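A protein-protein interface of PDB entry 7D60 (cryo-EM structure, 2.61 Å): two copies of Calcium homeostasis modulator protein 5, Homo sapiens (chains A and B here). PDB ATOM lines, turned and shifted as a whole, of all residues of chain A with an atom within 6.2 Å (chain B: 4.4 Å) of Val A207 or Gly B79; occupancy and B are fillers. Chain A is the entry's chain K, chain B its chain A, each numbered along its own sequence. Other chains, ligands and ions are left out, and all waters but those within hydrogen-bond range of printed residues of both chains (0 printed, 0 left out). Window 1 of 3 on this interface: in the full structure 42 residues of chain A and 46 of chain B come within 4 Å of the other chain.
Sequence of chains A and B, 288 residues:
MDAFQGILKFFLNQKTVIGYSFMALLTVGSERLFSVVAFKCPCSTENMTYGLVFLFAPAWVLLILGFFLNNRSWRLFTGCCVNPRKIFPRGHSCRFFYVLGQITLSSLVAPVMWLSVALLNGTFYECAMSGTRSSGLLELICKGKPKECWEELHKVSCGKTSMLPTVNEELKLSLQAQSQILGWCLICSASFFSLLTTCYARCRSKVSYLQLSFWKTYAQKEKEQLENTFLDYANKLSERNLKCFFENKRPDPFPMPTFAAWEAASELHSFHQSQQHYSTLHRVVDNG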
ATOM      1  N   ARG A 202     -12.380 -30.614 -17.051  1.00  0.00           N
ATOM      2  CA  ARG A 202     -12.866 -29.852 -15.909  1.00  0.00           C
ATOM      3  C   ARG A 202     -11.722 -29.240 -15.117  1.00  0.00           C
ATOM      4  O   ARG A 202     -11.861 -28.137 -14.587  1.00  0.00           O
ATOM      5  CB  ARG A 202     -13.710 -30.738 -15.002  1.00  0.00           C
ATOM      6  CG  ARG A 202     -14.928 -31.312 -15.663  1.00  0.00           C
ATOM      7  CD  ARG A 202     -15.989 -30.270 -15.861  1.00  0.00           C
ATOM      8  NE  ARG A 202     -16.651 -29.933 -14.609  1.00  0.00           N
ATOM      9  CZ  ARG A 202     -17.915 -30.226 -14.330  1.00  0.00           C
ATOM     10  NH1 ARG A 202     -18.655 -30.871 -15.219  1.00  0.00           N
ATOM     11  NH2 ARG A 202     -18.439 -29.876 -13.164  1.00  0.00           N
ATOM     12  N   CYS A 203     -10.588 -29.939 -15.020  1.00  0.00           N
ATOM     13  CA  CYS A 203      -9.432 -29.400 -14.314  1.00  0.00           C
ATOM     14  C   CYS A 203      -8.807 -28.225 -15.043  1.00  0.00           C
ATOM     15  O   CYS A 203      -8.115 -27.420 -14.417  1.00  0.00           O
ATOM     16  CB  CYS A 203      -8.369 -30.478 -14.113  1.00  0.00           C
ATOM     17  SG  CYS A 203      -8.663 -31.632 -12.767  1.00  0.00           S
ATOM     18  N   ARG A 204      -9.027 -28.112 -16.347  1.00  0.00           N
ATOM     19  CA  ARG A 204      -8.453 -27.052 -17.156  1.00  0.00           C
ATOM     20  C   ARG A 204      -9.480 -25.983 -17.509  1.00  0.00           C
ATOM     21  O   ARG A 204      -9.250 -25.183 -18.419  1.00  0.00           O
ATOM     22  CB  ARG A 204      -7.844 -27.648 -18.421  1.00  0.00           C
ATOM     23  CG  ARG A 204      -6.530 -27.042 -18.825  1.00  0.00           C
ATOM     24  CD  ARG A 204      -6.240 -27.365 -20.267  1.00  0.00           C
ATOM     25  NE  ARG A 204      -5.158 -26.553 -20.805  1.00  0.00           N
ATOM     26  CZ  ARG A 204      -4.917 -26.410 -22.103  1.00  0.00           C
ATOM     27  NH1 ARG A 204      -5.692 -27.015 -22.992  1.00  0.00           N
ATOM     28  NH2 ARG A 204      -3.909 -25.653 -22.512  1.00  0.00           N
ATOM     29  N   SER A 205     -10.607 -25.962 -16.808  1.00  0.00           N
ATOM     30  CA  SER A 205     -11.659 -24.997 -17.072  1.00  0.00           C
ATOM     31  C   SER A 205     -11.259 -23.610 -16.583  1.00  0.00           C
ATOM     32  O   SER A 205     -10.427 -23.457 -15.688  1.00  0.00           O
ATOM     33  CB  SER A 205     -12.950 -25.441 -16.397  1.00  0.00           C
ATOM     34  OG  SER A 205     -13.865 -24.377 -16.294  1.00  0.00           O
ATOM     35  N   LYS A 206     -11.858 -22.588 -17.195  1.00  0.00           N
ATOM     36  CA  LYS A 206     -11.530 -21.209 -16.861  1.00  0.00           C
ATOM     37  C   LYS A 206     -12.288 -20.699 -15.648  1.00  0.00           C
ATOM     38  O   LYS A 206     -11.850 -19.732 -15.021  1.00  0.00           O
ATOM     39  CB  LYS A 206     -11.813 -20.299 -18.052  1.00  0.00           C
ATOM     40  CG  LYS A 206     -10.895 -20.523 -19.224  1.00  0.00           C
ATOM     41  CD  LYS A 206      -9.478 -20.142 -18.868  1.00  0.00           C
ATOM     42  CE  LYS A 206      -8.626 -19.987 -20.108  1.00  0.00           C
ATOM     43  NZ  LYS A 206      -7.402 -20.828 -20.039  1.00  0.00           N
ATOM     44  N   VAL A 207     -13.411 -21.317 -15.309  1.00  0.00           N
ATOM     45  CA  VAL A 207     -14.241 -20.891 -14.197  1.00  0.00           C
ATOM     46  C   VAL A 207     -14.291 -22.013 -13.171  1.00  0.00           C
ATOM     47  O   VAL A 207     -13.990 -23.170 -13.463  1.00  0.00           O
ATOM     48  CB  VAL A 207     -15.657 -20.500 -14.661  1.00  0.00           C
ATOM     49  CG1 VAL A 207     -15.586 -19.374 -15.652  1.00  0.00           C
ATOM     50  CG2 VAL A 207     -16.355 -21.676 -15.282  1.00  0.00           C
ATOM     51  N   SER A 208     -14.674 -21.659 -11.952  1.00  0.00           N
ATOM     52  CA  SER A 208     -14.791 -22.629 -10.877  1.00  0.00           C
ATOM     53  C   SER A 208     -16.164 -23.286 -10.933  1.00  0.00           C
ATOM     54  O   SER A 208     -16.905 -23.129 -11.902  1.00  0.00           O
ATOM     55  CB  SER A 208     -14.522 -21.963  -9.536  1.00  0.00           C
ATOM     56  OG  SER A 208     -13.131 -21.854  -9.312  1.00  0.00           O
ATOM     57  N   TYR A 209     -16.516 -24.040  -9.894  1.00  0.00           N
ATOM     58  CA  TYR A 209     -17.723 -24.853  -9.948  1.00  0.00           C
ATOM     59  C   TYR A 209     -18.987 -24.010  -9.874  1.00  0.00           C
ATOM     60  O   TYR A 209     -19.997 -24.359 -10.491  1.00  0.00           O
ATOM     61  CB  TYR A 209     -17.717 -25.884  -8.818  1.00  0.00           C
ATOM     62  CG  TYR A 209     -18.984 -26.699  -8.762  1.00  0.00           C
ATOM     63  CD1 TYR A 209     -19.210 -27.718  -9.679  1.00  0.00           C
ATOM     64  CD2 TYR A 209     -19.972 -26.433  -7.818  1.00  0.00           C
ATOM     65  CE1 TYR A 209     -20.371 -28.461  -9.652  1.00  0.00           C
ATOM     66  CE2 TYR A 209     -21.145 -27.160  -7.794  1.00  0.00           C
ATOM     67  CZ  TYR A 209     -21.332 -28.179  -8.708  1.00  0.00           C
ATOM     68  OH  TYR A 209     -22.490 -28.917  -8.679  1.00  0.00           O
ATOM     69  N   GLN A 211     -19.513 -20.713 -10.762  1.00  0.00           N
ATOM     70  CA  GLN A 211     -19.763 -19.913 -11.950  1.00  0.00           C
ATOM     71  C   GLN A 211     -20.139 -20.781 -13.141  1.00  0.00           C
ATOM     72  O   GLN A 211     -20.872 -20.331 -14.024  1.00  0.00           O
ATOM     73  CB  GLN A 211     -18.537 -19.070 -12.275  1.00  0.00           C
ATOM     74  CG  GLN A 211     -18.836 -17.866 -13.110  1.00  0.00           C
ATOM     75  CD  GLN A 211     -17.628 -17.001 -13.323  1.00  0.00           C
ATOM     76  OE1 GLN A 211     -16.554 -17.284 -12.810  1.00  0.00           O
ATOM     77  NE2 GLN A 211     -17.794 -15.937 -14.087  1.00  0.00           N
ATOM     78  N   LEU A 212     -19.651 -22.017 -13.186  1.00  0.00           N
ATOM     79  CA  LEU A 212     -20.045 -22.941 -14.239  1.00  0.00           C
ATOM     80  C   LEU A 212     -21.476 -23.420 -14.068  1.00  0.00           C
ATOM     81  O   LEU A 212     -22.116 -23.791 -15.052  1.00  0.00           O
ATOM     82  CB  LEU A 212     -19.089 -24.130 -14.267  1.00  0.00           C
ATOM     83  CG  LEU A 212     -19.147 -25.090 -15.452  1.00  0.00           C
ATOM     84  CD1 LEU A 212     -18.502 -24.478 -16.665  1.00  0.00           C
ATOM     85  CD2 LEU A 212     -18.482 -26.387 -15.094  1.00  0.00           C
ATOM     86  N   TRP A 215     -23.542 -20.555 -15.558  1.00  0.00           N
ATOM     87  CA  TRP A 215     -23.365 -20.547 -17.004  1.00  0.00           C
ATOM     88  C   TRP A 215     -24.250 -21.590 -17.678  1.00  0.00           C
ATOM     89  O   TRP A 215     -24.798 -21.343 -18.755  1.00  0.00           O
ATOM     90  CB  TRP A 215     -21.885 -20.780 -17.302  1.00  0.00           C
ATOM     91  CG  TRP A 215     -21.394 -20.605 -18.704  1.00  0.00           C
ATOM     92  CD1 TRP A 215     -22.122 -20.323 -19.816  1.00  0.00           C
ATOM     93  CD2 TRP A 215     -20.035 -20.712 -19.137  1.00  0.00           C
ATOM     94  NE1 TRP A 215     -21.309 -20.255 -20.912  1.00  0.00           N
ATOM     95  CE2 TRP A 215     -20.019 -20.486 -20.520  1.00  0.00           C
ATOM     96  CE3 TRP A 215     -18.832 -20.978 -18.485  1.00  0.00           C
ATOM     97  CZ2 TRP A 215     -18.850 -20.517 -21.263  1.00  0.00           C
ATOM     98  CZ3 TRP A 215     -17.672 -21.008 -19.223  1.00  0.00           C
ATOM     99  CH2 TRP A 215     -17.688 -20.780 -20.596  1.00  0.00           C
ATOM    100  N   PHE A 271     -14.708 -18.213 -23.287  1.00  0.00           N
ATOM    101  CA  PHE A 271     -14.810 -17.391 -22.088  1.00  0.00           C
ATOM    102  C   PHE A 271     -13.540 -16.580 -21.861  1.00  0.00           C
ATOM    103  O   PHE A 271     -12.427 -17.055 -22.093  1.00  0.00           O
ATOM    104  CB  PHE A 271     -15.089 -18.265 -20.866  1.00  0.00           C
ATOM    105  CG  PHE A 271     -15.540 -17.493 -19.657  1.00  0.00           C
ATOM    106  CD1 PHE A 271     -16.878 -17.197 -19.469  1.00  0.00           C
ATOM    107  CD2 PHE A 271     -14.627 -17.068 -18.701  1.00  0.00           C
ATOM    108  CE1 PHE A 271     -17.296 -16.486 -18.363  1.00  0.00           C
ATOM    109  CE2 PHE A 271     -15.039 -16.352 -17.594  1.00  0.00           C
ATOM    110  CZ  PHE A 271     -16.374 -16.065 -17.425  1.00  0.00           C
ATOM    111  N   PHE B  77     -12.514 -30.384  -8.150  1.00  0.00           N
ATOM    112  CA  PHE B  77     -11.523 -30.344  -9.211  1.00  0.00           C
ATOM    113  C   PHE B  77     -11.803 -29.343 -10.322  1.00  0.00           C
ATOM    114  O   PHE B  77     -10.891 -29.059 -11.099  1.00  0.00           O
ATOM    115  CB  PHE B  77     -11.369 -31.735  -9.840  1.00  0.00           C
ATOM    116  CG  PHE B  77     -10.549 -32.679  -9.018  1.00  0.00           C
ATOM    117  CD1 PHE B  77      -9.245 -32.368  -8.681  1.00  0.00           C
ATOM    118  CD2 PHE B  77     -11.087 -33.873  -8.571  1.00  0.00           C
ATOM    119  CE1 PHE B  77      -8.490 -33.233  -7.917  1.00  0.00           C
ATOM    120  CE2 PHE B  77     -10.337 -34.739  -7.809  1.00  0.00           C
ATOM    121  CZ  PHE B  77      -9.038 -34.419  -7.483  1.00  0.00           C
ATOM    122  N   THR B  78     -13.019 -28.810 -10.426  1.00  0.00           N
ATOM    123  CA  THR B  78     -13.367 -27.922 -11.531  1.00  0.00           C
ATOM    124  C   THR B  78     -12.641 -26.592 -11.396  1.00  0.00           C
ATOM    125  O   THR B  78     -12.801 -25.888 -10.396  1.00  0.00           O
ATOM    126  CB  THR B  78     -14.871 -27.695 -11.578  1.00  0.00           C
ATOM    127  OG1 THR B  78     -15.541 -28.954 -11.653  1.00  0.00           O
ATOM    128  CG2 THR B  78     -15.241 -26.876 -12.780  1.00  0.00           C
ATOM    129  N   GLY B  79     -11.835 -26.254 -12.394  1.00  0.00           N
ATOM    130  CA  GLY B  79     -11.058 -25.036 -12.339  1.00  0.00           C
ATOM    131  C   GLY B  79      -9.815 -25.134 -11.494  1.00  0.00           C
ATOM    132  O   GLY B  79      -9.385 -24.130 -10.927  1.00  0.00           O
ATOM    133  N   CYS B  80      -9.220 -26.323 -11.403  1.00  0.00           N
ATOM    134  CA  CYS B  80      -8.086 -26.547 -10.512  1.00  0.00           C
ATOM    135  C   CYS B  80      -6.832 -25.832 -10.996  1.00  0.00           C
ATOM    136  O   CYS B  80      -6.118 -25.219 -10.197  1.00  0.00           O
ATOM    137  CB  CYS B  80      -7.827 -28.048 -10.382  1.00  0.00           C
ATOM    138  SG  CYS B  80      -6.243 -28.492  -9.657  1.00  0.00           S
ATOM    139  N   CYS B  81      -6.552 -25.882 -12.294  1.00  0.00           N
ATOM    140  CA  CYS B  81      -5.301 -25.361 -12.832  1.00  0.00           C
ATOM    141  C   CYS B  81      -5.277 -23.843 -12.977  1.00  0.00           C
ATOM    142  O   CYS B  81      -4.256 -23.303 -13.412  1.00  0.00           O
ATOM    143  CB  CYS B  81      -5.008 -26.009 -14.186  1.00  0.00           C
ATOM    144  SG  CYS B  81      -4.841 -27.804 -14.132  1.00  0.00           S
ATOM    145  N   VAL B  82      -6.363 -23.145 -12.644  1.00  0.00           N
ATOM    146  CA  VAL B  82      -6.327 -21.686 -12.605  1.00  0.00           C
ATOM    147  C   VAL B  82      -5.458 -21.216 -11.445  1.00  0.00           C
ATOM    148  O   VAL B  82      -4.550 -20.394 -11.615  1.00  0.00           O
ATOM    149  CB  VAL B  82      -7.755 -21.117 -12.511  1.00  0.00           C
ATOM    150  CG1 VAL B  82      -7.729 -19.645 -12.152  1.00  0.00           C
ATOM    151  CG2 VAL B  82      -8.491 -21.328 -13.815  1.00  0.00           C
ATOM    152  N   LYS B  86      -5.926 -22.858  -4.021  1.00  0.00           N
ATOM    153  CA  LYS B  86      -7.243 -22.854  -3.401  1.00  0.00           C
ATOM    154  C   LYS B  86      -7.732 -24.255  -3.066  1.00  0.00           C
ATOM    155  O   LYS B  86      -8.799 -24.395  -2.461  1.00  0.00           O
ATOM    156  CB  LYS B  86      -8.255 -22.154  -4.308  1.00  0.00           C
ATOM    157  CG  LYS B  86      -8.714 -22.978  -5.489  1.00  0.00           C
ATOM    158  CD  LYS B  86      -9.517 -22.132  -6.458  1.00  0.00           C
ATOM    159  CE  LYS B  86      -9.372 -22.642  -7.878  1.00  0.00           C
ATOM    160  NZ  LYS B  86     -10.183 -21.843  -8.829  1.00  0.00           N
ATOM    161  N   GLU B 263     -14.592 -16.847  -7.457  1.00  0.00           N
ATOM    162  CA  GLU B 263     -13.585 -17.851  -7.140  1.00  0.00           C
ATOM    163  C   GLU B 263     -13.352 -17.983  -5.644  1.00  0.00           C
ATOM    164  O   GLU B 263     -12.940 -19.050  -5.184  1.00  0.00           O
ATOM    165  CB  GLU B 263     -12.267 -17.523  -7.839  1.00  0.00           C
ATOM    166  CG  GLU B 263     -12.357 -17.441  -9.351  1.00  0.00           C
ATOM    167  CD  GLU B 263     -12.844 -18.727  -9.999  1.00  0.00           C
ATOM    168  OE1 GLU B 263     -12.063 -19.700 -10.046  1.00  0.00           O
ATOM    169  OE2 GLU B 263     -14.001 -18.762 -10.477  1.00  0.00           O
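O of Phe B77 touches O of Arg A202, 3.7 Å away. O of Ser A205 touches CA of Gly B79, 3.8 Å away. O of Ser A205 touches CG2 of Val B82 (3.4 Å). Val B82 touches Lys A206. Thr B78 touches Val A207. Val A207 touches Gly B79 (O to CA, 3.7 Å). Thr B78 touches Ser A208. Gln A211 touches Glu B263.
The side-chain amino group (NZ) of Lys B86 is in hydrogen-bond range of the backbone carbonyl oxygen (O) of Gly B79, 3.2 Å away. The side-chain amino group (NZ) of Lys B86 is in salt-bridge range of the side-chain carboxylate (OE1) of Glu B263 (3.1 Å). O of Val A207 is in hydrogen-bond range of OG of Ser A205.
Of the printed residues of chain B, Arg A202 touches Phe B77 (3.7 Å), Thr B78 (3.3 Å) and Gly B79 (2.9 Å). Arg A204 touches none of the printed residues of chain B. Of chain B, only Thr B78 and Gly B79 come within 4 Å of Val A207. Tyr A209 touches none of the printed residues of chain B. Of the printed residues of chain A, Phe B77 touches Arg A202 and Cys A203. Gly B79 touches just these residues of chain A: Arg A202, Ser A205 and Val A207. Printed residues of chain A within 4 Å of Cys B80: Cys A203 (3.4 Å). Of the printed residues of chain A, Cys B81 touches Cys A203. Of the printed residues of chain A, Lys B86 touches Ser A208 (3.0 Å). The nearest residue of chain B that does not touch Val A207 is Glu B263 (4.2 Å). The nearest residue of chain A that does not touch Gly B79 is Cys A203 (4.1 Å).
The side-chain amino group (NZ) of Lys B86 is in hydrogen-bond range of the side-chain hydroxyl (OG) of Ser A208 (3.0 Å). The backbone NH of Cys B81 is in hydrogen-bond range of the backbone carbonyl oxygen of Cys A203. The backbone carbonyl oxygen (O) of Phe B77 sits close to the side-chain sulfur (SG) of Cys A203, at 3.8 Å. The backbone NH (N) of Gly B79 sits at hydrogen-bond distance from the backbone carbonyl oxygen (O) of Arg A202. The side-chain hydroxyl (OG1) of Thr B78 sits at hydrogen-bond distance from the guanidinium group (NE) of Arg A202, 3.3 Å away. The side-chain hydroxyl (OG) of Ser A208 is in hydrogen-bond range of the side-chain carboxylate (OE1) of Glu B263, at 2.5 Å. N of Cys B80 lies within hydrogen-bond range of O of Cys A203 (3.4 Å).
Of the 8 printed residues of chain B, 8 touch a printed residue of chain A.
No position is printed for both chains. Of the 15 pairs that touch across the chains among the printed residues, none has its exchanged pair printed and touching as well.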
